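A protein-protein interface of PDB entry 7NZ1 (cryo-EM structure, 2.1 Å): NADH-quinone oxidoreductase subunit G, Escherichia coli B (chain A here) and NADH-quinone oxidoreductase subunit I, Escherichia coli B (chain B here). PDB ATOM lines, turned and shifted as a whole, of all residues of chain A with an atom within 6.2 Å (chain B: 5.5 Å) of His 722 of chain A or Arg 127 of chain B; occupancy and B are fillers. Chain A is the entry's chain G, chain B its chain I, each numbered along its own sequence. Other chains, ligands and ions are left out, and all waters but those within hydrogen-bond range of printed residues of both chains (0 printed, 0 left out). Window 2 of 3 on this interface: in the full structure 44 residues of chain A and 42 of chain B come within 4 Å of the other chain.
Of the 9 printed residues of chain B, 5 touch a printed residue of chain A.
Printed residues of chain B that touch a printed residue of chain A: Asn 95, Ser 97, Arg 127, Gln 128 and Val 131.
Of the 6 printed residues of chain A, 4 touch a printed residue of chain B.
Among the printed residues, 8 pairs touch across the chains.
Of chain B, only Arg 127 (3.1 Å) comes within 4 Å of His 722 of chain A.
Of chain A, only Val 721 and His 722 come within 4 Å of Arg 127 of chain B.
Of the printed residues of chain B, Ser 720 of chain A touches Gln 128 (3.4 Å).
Of the printed residues of chain A, Asn 95 of chain B touches Val 721 (3.5 Å) and Glu 723 (3.8 Å).
Printed residues of chain B within 4 Å of Val 721 of chain A: Asn 95, Ser 97, Arg 127, Gln 128 and Val 131.
Of the printed residues of chain A, Ser 97 of chain B touches Val 721 (3.9996 Å).
The nearest residue of chain A that does not touch Arg 127 of chain B is Glu 723 of chain A (4.8 Å).
The nearest printed residue of chain B that does not touch Glu 723 of chain A is Arg 127 of chain B (4.8 Å).
The backbone NH (N) of Val 721 of chain A sits at hydrogen-bond distance from the side-chain amide oxygen (OE1) of Gln 128 of chain B, 2.7 Å away.
The guanidinium group of Arg 127 of chain B sits at hydrogen-bond distance from a ring nitrogen (ND1) of His 722 of chain A (3.1 Å).
OG of Ser 97 of chain B sits at hydrogen-bond distance from OD1 of Asn 95 of chain B (2.8 Å).
OG of Ser 720 of chain A sits at hydrogen-bond distance from O of His 722 of chain A, at 3.0 Å.
NH1 of Arg 127 of chain B sits at hydrogen-bond distance from OG of Ser 97 of chain B, at 3.4 Å.
Among the printed residues, merely in contact across the chains: Ser 720 of chain A with Gln 128 of chain B (3.4 Å), Val 721 of chain A with Asn 95 of chain B (3.5 Å), Val 721 of chain A with Val 131 of chain B (3.7 Å), Val 721 of chain A with Arg 127 of chain B (3.8 Å), Glu 723 of chain A with Asn 95 of chain B (3.8 Å) and Val 721 of chain A with Ser 97 of chain B (3.9996 Å).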
ATOM      1  N   ARG A 716      -8.009 -31.060   8.953  1.00  0.00           N
ATOM      2  CA  ARG A 716      -7.893 -32.047  10.012  1.00  0.00           C
ATOM      3  C   ARG A 716      -7.444 -31.401  11.318  1.00  0.00           C
ATOM      4  O   ARG A 716      -6.941 -32.089  12.209  1.00  0.00           O
ATOM      5  CB  ARG A 716      -6.925 -33.160   9.593  1.00  0.00           C
ATOM      6  CG  ARG A 716      -7.294 -34.545  10.099  1.00  0.00           C
ATOM      7  CD  ARG A 716      -6.260 -35.600   9.717  1.00  0.00           C
ATOM      8  NE  ARG A 716      -5.062 -35.521  10.544  1.00  0.00           N
ATOM      9  CZ  ARG A 716      -4.944 -36.035  11.763  1.00  0.00           C
ATOM     10  NH1 ARG A 716      -5.936 -36.700  12.335  1.00  0.00           N
ATOM     11  NH2 ARG A 716      -3.802 -35.876  12.423  1.00  0.00           N
ATOM     12  N   SER A 720      -6.083 -33.091  15.250  1.00  0.00           N
ATOM     13  CA  SER A 720      -4.721 -32.720  15.604  1.00  0.00           C
ATOM     14  C   SER A 720      -4.319 -31.477  14.826  1.00  0.00           C
ATOM     15  O   SER A 720      -4.482 -31.426  13.605  1.00  0.00           O
ATOM     16  CB  SER A 720      -3.741 -33.865  15.322  1.00  0.00           C
ATOM     17  OG  SER A 720      -2.433 -33.376  15.091  1.00  0.00           O
ATOM     18  N   VAL A 721      -3.764 -30.489  15.537  1.00  0.00           N
ATOM     19  CA  VAL A 721      -3.284 -29.273  14.890  1.00  0.00           C
ATOM     20  C   VAL A 721      -2.005 -29.535  14.097  1.00  0.00           C
ATOM     21  O   VAL A 721      -1.695 -28.793  13.158  1.00  0.00           O
ATOM     22  CB  VAL A 721      -3.118 -28.161  15.954  1.00  0.00           C
ATOM     23  CG1 VAL A 721      -1.929 -28.425  16.871  1.00  0.00           C
ATOM     24  CG2 VAL A 721      -3.043 -26.773  15.324  1.00  0.00           C
ATOM     25  N   HIS A 722      -1.276 -30.602  14.418  1.00  0.00           N
ATOM     26  CA  HIS A 722      -0.108 -30.995  13.645  1.00  0.00           C
ATOM     27  C   HIS A 722      -0.571 -31.640  12.349  1.00  0.00           C
ATOM     28  O   HIS A 722      -1.317 -32.625  12.382  1.00  0.00           O
ATOM     29  CB  HIS A 722       0.764 -31.956  14.449  1.00  0.00           C
ATOM     30  CG  HIS A 722       1.040 -31.486  15.841  1.00  0.00           C
ATOM     31  ND1 HIS A 722       2.036 -30.582  16.135  1.00  0.00           N
ATOM     32  CD2 HIS A 722       0.449 -31.793  17.020  1.00  0.00           C
ATOM     33  CE1 HIS A 722       2.042 -30.347  17.435  1.00  0.00           C
ATOM     34  NE2 HIS A 722       1.092 -31.071  17.996  1.00  0.00           N
ATOM     35  N   GLU A 723      -0.171 -31.052  11.220  1.00  0.00           N
ATOM     36  CA  GLU A 723      -0.601 -31.546   9.913  1.00  0.00           C
ATOM     37  C   GLU A 723      -0.029 -32.938   9.670  1.00  0.00           C
ATOM     38  O   GLU A 723       1.169 -33.156   9.880  1.00  0.00           O
ATOM     39  CB  GLU A 723      -0.161 -30.606   8.780  1.00  0.00           C
ATOM     40  CG  GLU A 723      -0.881 -29.246   8.659  1.00  0.00           C
ATOM     41  CD  GLU A 723      -0.535 -28.251   9.764  1.00  0.00           C
ATOM     42  OE1 GLU A 723       0.503 -28.432  10.435  1.00  0.00           O
ATOM     43  OE2 GLU A 723      -1.297 -27.278   9.956  1.00  0.00           O
ATOM     44  N   PRO A 724      -0.840 -33.899   9.250  1.00  0.00           N
ATOM     45  CA  PRO A 724      -0.320 -35.232   8.954  1.00  0.00           C
ATOM     46  C   PRO A 724       0.382 -35.234   7.605  1.00  0.00           C
ATOM     47  O   PRO A 724       0.304 -34.278   6.832  1.00  0.00           O
ATOM     48  CB  PRO A 724      -1.584 -36.087   8.935  1.00  0.00           C
ATOM     49  CG  PRO A 724      -2.572 -35.165   8.316  1.00  0.00           C
ATOM     50  CD  PRO A 724      -2.283 -33.818   8.959  1.00  0.00           C
ATOM     51  N   ASN B  95      -7.486 -21.999  11.973  1.00  0.00           N
ATOM     52  CA  ASN B  95      -6.262 -22.398  12.668  1.00  0.00           C
ATOM     53  C   ASN B  95      -5.395 -21.159  12.862  1.00  0.00           C
ATOM     54  O   ASN B  95      -4.663 -20.750  11.958  1.00  0.00           O
ATOM     55  CB  ASN B  95      -5.542 -23.488  11.878  1.00  0.00           C
ATOM     56  CG  ASN B  95      -4.306 -24.028  12.584  1.00  0.00           C
ATOM     57  OD1 ASN B  95      -4.114 -23.836  13.779  1.00  0.00           O
ATOM     58  ND2 ASN B  95      -3.485 -24.753  11.841  1.00  0.00           N
ATOM     59  N   SER B  97      -2.797 -20.744  14.668  1.00  0.00           N
ATOM     60  CA  SER B  97      -1.356 -20.968  14.691  1.00  0.00           C
ATOM     61  C   SER B  97      -0.748 -20.675  13.322  1.00  0.00           C
ATOM     62  O   SER B  97       0.380 -20.185  13.232  1.00  0.00           O
ATOM     63  CB  SER B  97      -1.039 -22.394  15.142  1.00  0.00           C
ATOM     64  OG  SER B  97      -1.364 -23.340  14.144  1.00  0.00           O
ATOM     65  N   TYR B 125      -1.362 -22.183  26.105  1.00  0.00           N
ATOM     66  CA  TYR B 125      -0.372 -23.188  26.474  1.00  0.00           C
ATOM     67  C   TYR B 125      -0.295 -24.317  25.461  1.00  0.00           C
ATOM     68  O   TYR B 125       0.754 -24.952  25.332  1.00  0.00           O
ATOM     69  CB  TYR B 125      -0.676 -23.771  27.855  1.00  0.00           C
ATOM     70  CG  TYR B 125      -0.815 -22.735  28.935  1.00  0.00           C
ATOM     71  CD1 TYR B 125       0.238 -21.875  29.234  1.00  0.00           C
ATOM     72  CD2 TYR B 125      -1.998 -22.607  29.648  1.00  0.00           C
ATOM     73  CE1 TYR B 125       0.112 -20.918  30.212  1.00  0.00           C
ATOM     74  CE2 TYR B 125      -2.131 -21.654  30.636  1.00  0.00           C
ATOM     75  CZ  TYR B 125      -1.071 -20.816  30.915  1.00  0.00           C
ATOM     76  OH  TYR B 125      -1.204 -19.865  31.896  1.00  0.00           O
ATOM     77  N   LYS B 126      -1.381 -24.581  24.745  1.00  0.00           N
ATOM     78  CA  LYS B 126      -1.458 -25.683  23.800  1.00  0.00           C
ATOM     79  C   LYS B 126      -1.756 -25.130  22.418  1.00  0.00           C
ATOM     80  O   LYS B 126      -2.551 -24.198  22.273  1.00  0.00           O
ATOM     81  CB  LYS B 126      -2.543 -26.686  24.204  1.00  0.00           C
ATOM     82  CG  LYS B 126      -2.486 -27.141  25.647  1.00  0.00           C
ATOM     83  CD  LYS B 126      -1.328 -28.086  25.897  1.00  0.00           C
ATOM     84  CE  LYS B 126      -1.354 -28.626  27.314  1.00  0.00           C
ATOM     85  NZ  LYS B 126      -1.146 -27.558  28.331  1.00  0.00           N
ATOM     86  N   ARG B 127      -1.111 -25.711  21.402  1.00  0.00           N
ATOM     87  CA  ARG B 127      -1.365 -25.296  20.026  1.00  0.00           C
ATOM     88  C   ARG B 127      -2.756 -25.715  19.561  1.00  0.00           C
ATOM     89  O   ARG B 127      -3.354 -25.031  18.721  1.00  0.00           O
ATOM     90  CB  ARG B 127      -0.286 -25.869  19.104  1.00  0.00           C
ATOM     91  CG  ARG B 127      -0.176 -25.189  17.753  1.00  0.00           C
ATOM     92  CD  ARG B 127       1.260 -25.102  17.290  1.00  0.00           C
ATOM     93  NE  ARG B 127       1.731 -26.326  16.652  1.00  0.00           N
ATOM     94  CZ  ARG B 127       1.594 -26.599  15.363  1.00  0.00           C
ATOM     95  NH1 ARG B 127       0.977 -25.766  14.546  1.00  0.00           N
ATOM     96  NH2 ARG B 127       2.088 -27.736  14.882  1.00  0.00           N
ATOM     97  N   GLN B 128      -3.300 -26.793  20.144  1.00  0.00           N
ATOM     98  CA  GLN B 128      -4.654 -27.253  19.835  1.00  0.00           C
ATOM     99  C   GLN B 128      -5.710 -26.234  20.244  1.00  0.00           C
ATOM    100  O   GLN B 128      -6.783 -26.173  19.637  1.00  0.00           O
ATOM    101  CB  GLN B 128      -4.921 -28.585  20.539  1.00  0.00           C
ATOM    102  CG  GLN B 128      -6.011 -29.471  19.936  1.00  0.00           C
ATOM    103  CD  GLN B 128      -6.069 -29.429  18.424  1.00  0.00           C
ATOM    104  OE1 GLN B 128      -5.242 -30.034  17.745  1.00  0.00           O
ATOM    105  NE2 GLN B 128      -7.063 -28.726  17.887  1.00  0.00           N
ATOM    106  N   ASP B 129      -5.416 -25.413  21.245  1.00  0.00           N
ATOM    107  CA  ASP B 129      -6.321 -24.355  21.663  1.00  0.00           C
ATOM    108  C   ASP B 129      -6.206 -23.106  20.801  1.00  0.00           C
ATOM    109  O   ASP B 129      -6.949 -22.148  21.026  1.00  0.00           O
ATOM    110  CB  ASP B 129      -6.066 -24.014  23.129  1.00  0.00           C
ATOM    111  CG  ASP B 129      -6.232 -25.218  24.034  1.00  0.00           C
ATOM    112  OD1 ASP B 129      -6.257 -26.353  23.508  1.00  0.00           O
ATOM    113  OD2 ASP B 129      -6.342 -25.036  25.260  1.00  0.00           O
ATOM    114  N   LEU B 130      -5.300 -23.088  19.823  1.00  0.00           N
ATOM    115  CA  LEU B 130      -5.308 -22.016  18.840  1.00  0.00           C
ATOM    116  C   LEU B 130      -6.284 -22.279  17.701  1.00  0.00           C
ATOM    117  O   LEU B 130      -6.495 -21.391  16.871  1.00  0.00           O
ATOM    118  CB  LEU B 130      -3.899 -21.794  18.290  1.00  0.00           C
ATOM    119  CG  LEU B 130      -2.932 -21.124  19.268  1.00  0.00           C
ATOM    120  CD1 LEU B 130      -1.522 -21.069  18.706  1.00  0.00           C
ATOM    121  CD2 LEU B 130      -3.428 -19.735  19.615  1.00  0.00           C
ATOM    122  N   VAL B 131      -6.888 -23.460  17.653  1.00  0.00           N
ATOM    123  CA  VAL B 131      -7.901 -23.792  16.660  1.00  0.00           C
ATOM    124  C   VAL B 131      -9.252 -23.298  17.162  1.00  0.00           C
ATOM    125  O   VAL B 131      -9.759 -23.775  18.183  1.00  0.00           O
ATOM    126  CB  VAL B 131      -7.930 -25.300  16.382  1.00  0.00           C
ATOM    127  CG1 VAL B 131      -9.078 -25.648  15.474  1.00  0.00           C
ATOM    128  CG2 VAL B 131      -6.616 -25.744  15.775  1.00  0.00           C
